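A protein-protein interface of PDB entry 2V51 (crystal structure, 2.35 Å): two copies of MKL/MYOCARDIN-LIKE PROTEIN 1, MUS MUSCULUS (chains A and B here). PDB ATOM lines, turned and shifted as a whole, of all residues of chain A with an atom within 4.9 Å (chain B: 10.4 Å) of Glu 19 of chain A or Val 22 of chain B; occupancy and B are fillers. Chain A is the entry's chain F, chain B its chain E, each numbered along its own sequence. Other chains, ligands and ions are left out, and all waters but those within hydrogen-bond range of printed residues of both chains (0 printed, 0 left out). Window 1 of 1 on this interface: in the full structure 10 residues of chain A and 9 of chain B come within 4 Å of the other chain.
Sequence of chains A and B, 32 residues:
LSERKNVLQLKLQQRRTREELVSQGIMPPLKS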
ATOM      1  N   THR A  17      10.915   1.663  33.410  1.00  0.00           N
ATOM      2  CA  THR A  17      12.376   1.964  33.425  1.00  0.00           C
ATOM      3  C   THR A  17      12.655   3.456  33.229  1.00  0.00           C
ATOM      4  O   THR A  17      11.922   4.139  32.478  1.00  0.00           O
ATOM      5  CB  THR A  17      13.125   1.288  32.258  1.00  0.00           C
ATOM      6  OG1 THR A  17      12.757  -0.085  32.181  1.00  0.00           O
ATOM      7  CG2 THR A  17      14.645   1.392  32.432  1.00  0.00           C
ATOM      8  N   ARG A  18      13.723   3.957  33.865  1.00  0.00           N
ATOM      9  CA  ARG A  18      14.233   5.291  33.533  1.00  0.00           C
ATOM     10  C   ARG A  18      14.341   5.435  32.008  1.00  0.00           C
ATOM     11  O   ARG A  18      13.747   6.357  31.434  1.00  0.00           O
ATOM     12  CB  ARG A  18      15.588   5.539  34.180  1.00  0.00           C
ATOM     13  CG  ARG A  18      15.531   5.903  35.630  1.00  0.00           C
ATOM     14  CD  ARG A  18      16.853   6.499  36.098  1.00  0.00           C
ATOM     15  NE  ARG A  18      17.242   7.670  35.297  1.00  0.00           N
ATOM     16  CZ  ARG A  18      17.071   8.941  35.651  1.00  0.00           C
ATOM     17  NH1 ARG A  18      16.506   9.236  36.814  1.00  0.00           N
ATOM     18  NH2 ARG A  18      17.471   9.918  34.832  1.00  0.00           N
ATOM     19  N   GLU A  19      15.068   4.503  31.368  1.00  0.00           N
ATOM     20  CA  GLU A  19      15.179   4.457  29.897  1.00  0.00           C
ATOM     21  C   GLU A  19      13.798   4.479  29.196  1.00  0.00           C
ATOM     22  O   GLU A  19      13.592   5.278  28.281  1.00  0.00           O
ATOM     23  CB  GLU A  19      16.060   3.275  29.408  1.00  0.00           C
ATOM     24  CG  GLU A  19      17.454   3.348  29.972  1.00  0.00           C
ATOM     25  CD  GLU A  19      18.460   2.354  29.373  1.00  0.00           C
ATOM     26  OE1 GLU A  19      18.208   1.762  28.308  1.00  0.00           O
ATOM     27  OE2 GLU A  19      19.541   2.193  29.984  1.00  0.00           O
ATOM     28  N   GLU A  20      12.859   3.625  29.620  1.00  0.00           N
ATOM     29  CA  GLU A  20      11.499   3.691  29.066  1.00  0.00           C
ATOM     30  C   GLU A  20      10.960   5.140  29.122  1.00  0.00           C
ATOM     31  O   GLU A  20      10.383   5.595  28.141  1.00  0.00           O
ATOM     32  CB  GLU A  20      10.515   2.705  29.734  1.00  0.00           C
ATOM     33  CG  GLU A  20      10.794   1.190  29.493  1.00  0.00           C
ATOM     34  CD  GLU A  20       9.701   0.242  30.060  1.00  0.00           C
ATOM     35  OE1 GLU A  20       8.962  -0.370  29.252  1.00  0.00           O
ATOM     36  OE2 GLU A  20       9.571   0.092  31.300  1.00  0.00           O
ATOM     37  N   LEU A  21      11.189   5.878  30.218  1.00  0.00           N
ATOM     38  CA  LEU A  21      10.642   7.240  30.309  1.00  0.00           C
ATOM     39  C   LEU A  21      11.388   8.267  29.489  1.00  0.00           C
ATOM     40  O   LEU A  21      10.770   9.190  28.958  1.00  0.00           O
ATOM     41  CB  LEU A  21      10.540   7.737  31.755  1.00  0.00           C
ATOM     42  CG  LEU A  21       9.823   6.819  32.717  1.00  0.00           C
ATOM     43  CD1 LEU A  21       9.754   7.562  33.986  1.00  0.00           C
ATOM     44  CD2 LEU A  21       8.430   6.411  32.160  1.00  0.00           C
ATOM     45  N   VAL A  22      12.715   8.142  29.430  1.00  0.00           N
ATOM     46  CA  VAL A  22      13.520   9.014  28.569  1.00  0.00           C
ATOM     47  C   VAL A  22      12.982   8.910  27.135  1.00  0.00           C
ATOM     48  O   VAL A  22      12.755   9.952  26.497  1.00  0.00           O
ATOM     49  CB  VAL A  22      15.053   8.717  28.626  1.00  0.00           C
ATOM     50  CG1 VAL A  22      15.836   9.676  27.742  1.00  0.00           C
ATOM     51  CG2 VAL A  22      15.560   8.845  30.030  1.00  0.00           C
ATOM     52  N   SER A  23      12.696   7.683  26.681  1.00  0.00           N
ATOM     53  CA  SER A  23      12.256   7.455  25.300  1.00  0.00           C
ATOM     54  C   SER A  23      10.805   7.851  25.020  1.00  0.00           C
ATOM     55  O   SER A  23      10.434   8.109  23.849  1.00  0.00           O
ATOM     56  CB  SER A  23      12.460   6.010  24.871  1.00  0.00           C
ATOM     57  OG  SER A  23      11.504   5.202  25.519  1.00  0.00           O
ATOM     58  N   ARG B  16      28.892   8.364  25.747  1.00  0.00           N
ATOM     59  CA  ARG B  16      27.658   8.891  26.227  1.00  0.00           C
ATOM     60  C   ARG B  16      26.908   7.826  27.027  1.00  0.00           C
ATOM     61  O   ARG B  16      27.164   6.630  26.880  1.00  0.00           O
ATOM     62  CB  ARG B  16      26.849   9.391  25.037  1.00  0.00           C
ATOM     63  CG  ARG B  16      27.427  10.652  24.433  1.00  0.00           C
ATOM     64  CD  ARG B  16      26.482  11.309  23.464  1.00  0.00           C
ATOM     65  NE  ARG B  16      26.661  10.758  22.127  1.00  0.00           N
ATOM     66  CZ  ARG B  16      25.666  10.440  21.300  1.00  0.00           C
ATOM     67  NH1 ARG B  16      24.382  10.594  21.696  1.00  0.00           N
ATOM     68  NH2 ARG B  16      25.959   9.946  20.088  1.00  0.00           N
ATOM     69  N   THR B  17      26.006   8.302  27.903  1.00  0.00           N
ATOM     70  CA  THR B  17      25.071   7.490  28.710  1.00  0.00           C
ATOM     71  C   THR B  17      24.140   6.679  27.811  1.00  0.00           C
ATOM     72  O   THR B  17      23.741   7.148  26.728  1.00  0.00           O
ATOM     73  CB  THR B  17      24.192   8.398  29.584  1.00  0.00           C
ATOM     74  OG1 THR B  17      25.030   9.180  30.436  1.00  0.00           O
ATOM     75  CG2 THR B  17      23.248   7.599  30.474  1.00  0.00           C
ATOM     76  N   ARG B  18      23.801   5.461  28.234  1.00  0.00           N
ATOM     77  CA  ARG B  18      22.657   4.784  27.631  1.00  0.00           C
ATOM     78  C   ARG B  18      21.467   5.741  27.484  1.00  0.00           C
ATOM     79  O   ARG B  18      20.962   5.924  26.386  1.00  0.00           O
ATOM     80  CB  ARG B  18      22.215   3.600  28.465  1.00  0.00           C
ATOM     81  CG  ARG B  18      23.265   2.586  28.761  1.00  0.00           C
ATOM     82  CD  ARG B  18      22.588   1.221  28.771  1.00  0.00           C
ATOM     83  NE  ARG B  18      21.385   1.195  27.921  1.00  0.00           N
ATOM     84  CZ  ARG B  18      20.885   0.095  27.367  1.00  0.00           C
ATOM     85  NH1 ARG B  18      21.505  -1.048  27.555  1.00  0.00           N
ATOM     86  NH2 ARG B  18      19.781   0.134  26.614  1.00  0.00           N
ATOM     87  N   GLU B  19      21.032   6.354  28.582  1.00  0.00           N
ATOM     88  CA  GLU B  19      19.944   7.350  28.516  1.00  0.00           C
ATOM     89  C   GLU B  19      20.145   8.433  27.425  1.00  0.00           C
ATOM     90  O   GLU B  19      19.211   8.683  26.643  1.00  0.00           O
ATOM     91  CB  GLU B  19      19.634   7.994  29.890  1.00  0.00           C
ATOM     92  CG  GLU B  19      19.165   7.035  30.946  1.00  0.00           C
ATOM     93  CD  GLU B  19      18.584   7.736  32.159  1.00  0.00           C
ATOM     94  OE1 GLU B  19      18.237   8.938  32.076  1.00  0.00           O
ATOM     95  OE2 GLU B  19      18.456   7.070  33.204  1.00  0.00           O
ATOM     96  N   GLU B  20      21.331   9.064  27.365  1.00  0.00           N
ATOM     97  CA  GLU B  20      21.627  10.061  26.314  1.00  0.00           C
ATOM     98  C   GLU B  20      21.305   9.442  24.954  1.00  0.00           C
ATOM     99  O   GLU B  20      20.731  10.104  24.103  1.00  0.00           O
ATOM    100  CB  GLU B  20      23.081  10.595  26.363  1.00  0.00           C
ATOM    101  CG  GLU B  20      23.474  11.352  27.675  1.00  0.00           C
ATOM    102  CD  GLU B  20      24.850  12.087  27.644  1.00  0.00           C
ATOM    103  OE1 GLU B  20      24.866  13.333  27.662  1.00  0.00           O
ATOM    104  OE2 GLU B  20      25.915  11.436  27.637  1.00  0.00           O
ATOM    105  N   LEU B  21      21.614   8.157  24.763  1.00  0.00           N
ATOM    106  CA  LEU B  21      21.371   7.499  23.476  1.00  0.00           C
ATOM    107  C   LEU B  21      19.926   7.135  23.228  1.00  0.00           C
ATOM    108  O   LEU B  21      19.490   7.105  22.072  1.00  0.00           O
ATOM    109  CB  LEU B  21      22.185   6.221  23.329  1.00  0.00           C
ATOM    110  CG  LEU B  21      23.678   6.258  23.183  1.00  0.00           C
ATOM    111  CD1 LEU B  21      23.977   4.869  22.673  1.00  0.00           C
ATOM    112  CD2 LEU B  21      24.093   7.364  22.214  1.00  0.00           C
ATOM    113  N   VAL B  22      19.202   6.787  24.295  1.00  0.00           N
ATOM    114  CA  VAL B  22      17.775   6.484  24.151  1.00  0.00           C
ATOM    115  C   VAL B  22      17.086   7.769  23.692  1.00  0.00           C
ATOM    116  O   VAL B  22      16.391   7.771  22.660  1.00  0.00           O
ATOM    117  CB  VAL B  22      17.151   5.902  25.419  1.00  0.00           C
ATOM    118  CG1 VAL B  22      15.700   5.690  25.215  1.00  0.00           C
ATOM    119  CG2 VAL B  22      17.776   4.574  25.746  1.00  0.00           C
ATOM    120  N   SER B  23      17.355   8.855  24.417  1.00  0.00           N
ATOM    121  CA  SER B  23      16.924  10.194  24.048  1.00  0.00           C
ATOM    122  C   SER B  23      17.288  10.568  22.610  1.00  0.00           C
ATOM    123  O   SER B  23      16.433  11.095  21.879  1.00  0.00           O
ATOM    124  CB  SER B  23      17.552  11.205  24.985  1.00  0.00           C
ATOM    125  OG  SER B  23      17.852  12.414  24.301  1.00  0.00           O
ATOM    126  N   GLN B  24      18.538  10.305  22.200  1.00  0.00           N
ATOM    127  CA  GLN B  24      18.973  10.649  20.826  1.00  0.00           C
ATOM    128  C   GLN B  24      18.229   9.848  19.746  1.00  0.00           C
ATOM    129  O   GLN B  24      18.337  10.178  18.580  1.00  0.00           O
ATOM    130  CB  GLN B  24      20.497  10.563  20.636  1.00  0.00           C
ATOM    131  N   GLY B  25      17.442   8.836  20.136  1.00  0.00           N
ATOM    132  CA  GLY B  25      16.762   7.943  19.165  1.00  0.00           C
ATOM    133  C   GLY B  25      17.633   6.811  18.586  1.00  0.00           C
ATOM    134  O   GLY B  25      17.216   6.083  17.674  1.00  0.00           O
ATOM    135  N   ILE B  26      18.836   6.655  19.144  1.00  0.00           N
ATOM    136  CA  ILE B  26      19.801   5.632  18.757  1.00  0.00           C
ATOM    137  C   ILE B  26      19.509   4.232  19.385  1.00  0.00           C
ATOM    138  O   ILE B  26      19.376   3.253  18.650  1.00  0.00           O
ATOM    139  CB  ILE B  26      21.249   6.174  19.024  1.00  0.00           C
ATOM    140  CG1 ILE B  26      21.521   7.390  18.124  1.00  0.00           C
ATOM    141  CG2 ILE B  26      22.321   5.091  18.852  1.00  0.00           C
ATOM    142  CD1 ILE B  26      22.675   8.246  18.552  1.00  0.00           C
ATOM    143  N   MET B  27      19.415   4.157  20.718  1.00  0.00           N
ATOM    144  CA  MET B  27      19.053   2.936  21.499  1.00  0.00           C
ATOM    145  C   MET B  27      17.528   2.782  21.773  1.00  0.00           C
ATOM    146  O   MET B  27      16.907   3.738  22.246  1.00  0.00           O
ATOM    147  CB  MET B  27      19.731   2.999  22.902  1.00  0.00           C
ATOM    148  CG  MET B  27      21.048   2.259  23.085  1.00  0.00           C
ATOM    149  SD  MET B  27      21.028   0.535  23.721  1.00  0.00           S
ATOM    150  CE  MET B  27      19.512  -0.186  23.097  1.00  0.00           C
ATOM    151  N   PRO B  28      16.937   1.580  21.545  1.00  0.00           N
ATOM    152  CA  PRO B  28      15.598   1.345  22.105  1.00  0.00           C
ATOM    153  C   PRO B  28      15.718   1.170  23.644  1.00  0.00           C
ATOM    154  O   PRO B  28      16.734   0.617  24.113  1.00  0.00           O
ATOM    155  CB  PRO B  28      15.167   0.035  21.444  1.00  0.00           C
ATOM    156  CG  PRO B  28      16.449  -0.694  21.214  1.00  0.00           C
ATOM    157  CD  PRO B  28      17.466   0.375  20.878  1.00  0.00           C
ATOM    158  N   PRO B  29      14.713   1.646  24.421  1.00  0.00           N
ATOM    159  CA  PRO B  29      14.833   1.726  25.888  1.00  0.00           C
ATOM    160  C   PRO B  29      15.192   0.422  26.635  1.00  0.00           C
ATOM    161  O   PRO B  29      16.237   0.362  27.302  1.00  0.00           O
ATOM    162  CB  PRO B  29      13.453   2.246  26.342  1.00  0.00           C
ATOM    163  CG  PRO B  29      12.562   2.177  25.139  1.00  0.00           C
ATOM    164  CD  PRO B  29      13.450   2.246  23.944  1.00  0.00           C
ATOM    165  N   LEU B  30      14.339  -0.597  26.536  1.00  0.00           N
ATOM    166  CA  LEU B  30      14.430  -1.810  27.385  1.00  0.00           C
ATOM    167  C   LEU B  30      13.372  -1.748  28.489  1.00  0.00           C
ATOM    168  O   LEU B  30      13.474  -0.906  29.387  1.00  0.00           O
ATOM    169  CB  LEU B  30      15.837  -2.040  28.005  1.00  0.00           C
ATOM    170  N   LYS B  31      12.377  -2.641  28.391  1.00  0.00           N
ATOM    171  CA  LYS B  31      11.268  -2.778  29.345  1.00  0.00           C
ATOM    172  C   LYS B  31      11.668  -3.500  30.640  1.00  0.00           C
ATOM    173  O   LYS B  31      12.816  -3.931  30.803  1.00  0.00           O
ATOM    174  CB  LYS B  31      10.092  -3.519  28.689  1.00  0.00           C
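NH2 of Arg 18 of chain B is in salt-bridge range of OE1 of Glu 19 of chain A (2.8 Å).
OE2 of Glu 19 of chain B lies within salt-bridge range of NE of Arg 18 of chain A, 2.5 Å away.
O of Pro 29 of chain B lies close to OE1 of Glu 19 of chain A, at 2.6 Å.
The side-chain hydroxyl (OG1) of Thr 17 of chain A lies within hydrogen-bond range of the backbone carbonyl oxygen (O) of Leu 30 of chain B (3.0 Å).
Arg 18 of chain A touches Glu 19 of chain B, and with the chains exchanged Glu 19 of chain A touches Arg 18 of chain B.
Glu 19 of chain A touches Val 22 of chain B, and with the chains exchanged Val 22 of chain A touches Glu 19 of chain B.
Val 22 of chain A touches Ser 23 of chain B, and with the chains exchanged Ser 23 of chain A touches Val 22 of chain B.
Positions printed for both chains: 17, 18, 19, 20, 21, 22 and 23.
Of the 13 pairs that touch across the chains among the printed residues, 6 have their exchanged pair printed and touching as well.
The side-chain sulfur (SD) of Met 27 of chain B lies within hydrogen-bond range of the guanidinium group (NH2) of Arg 18 of chain B (3.2 Å).
OE2 of Glu 20 of chain A is in hydrogen-bond range of N of Thr 17 of chain A.
The side-chain hydroxyl (OG) of Ser 23 of chain A lies within hydrogen-bond range of the backbone carbonyl oxygen (O) of Glu 19 of chain A, 3.5 Å away.
O of Glu 20 of chain A lies within hydrogen-bond range of OG of Ser 23 of chain A (2.9 Å).
Printed residues of chain A that touch a printed residue of chain B: Thr 17, Arg 18, Glu 19, Glu 20, Val 22 and Ser 23.
Hydrophobic or aromatic side chains of chain A that line the printed part of chain B: Val 22.
Among the printed residues, 13 pairs touch across the chains.
Among the printed residues, Asp or Glu carboxylates within 4 Å of a Lys or Arg side-chain nitrogen of the other chain: Arg 18 of chain A with Glu 19 of chain B and Glu 19 of chain A with Arg 18 of chain B.
Of chain B, only Arg 18, Val 22 and Pro 29 come within 4 Å of Glu 19 of chain A.
Of chain A, only Glu 19 and Ser 23 come within 4 Å of Val 22 of chain B.
Of chain B, only Glu 19 (3.4 Å) and Ser 23 (3.6 Å) come within 4 Å of Val 22 of chain A.
Of chain B, only Val 22 (3.3 Å) and Pro 29 (3.2 Å) come within 4 Å of Ser 23 of chain A.
Printed residues of chain A within 4 Å of Glu 19 of chain B: Arg 18 and Val 22.
Printed residues of chain A within 4 Å of Lys 31 of chain B: Thr 17 and Glu 20.
Printed residues of chain A within 4 Å of Ser 23 of chain B: Val 22 (3.6 Å).
Of the printed residues of chain A, Arg 18 of chain B touches Glu 19 (2.8 Å).
Of the printed residues of chain B, Arg 18 of chain A touches Glu 19.
Pro 28 of chain B touches none of the printed residues of chain A.
The nearest residue of chain B that does not touch Glu 19 of chain A is Glu 19 of chain B (4.2 Å).
OG1 of Thr 17 of chain A touches C of Lys 31 of chain B, 3.9 Å away.
Glu 19 of chain A touches Val 22 of chain B.
Pro 29 of chain B touches Glu 20 of chain A.
Leu 30 of chain B touches Glu 20 of chain A.
Lys 31 of chain B touches Glu 20 of chain A (CA to OE1, 3.3 Å).
Val 22 of chain A touches Glu 19 of chain B.
Val 22 of chain A touches Ser 23 of chain B.
CG1 of Val 22 of chain B touches CB of Ser 23 of chain A, 3.3 Å away.
Pro 29 of chain B touches Ser 23 of chain A (CG to OG, 3.2 Å).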
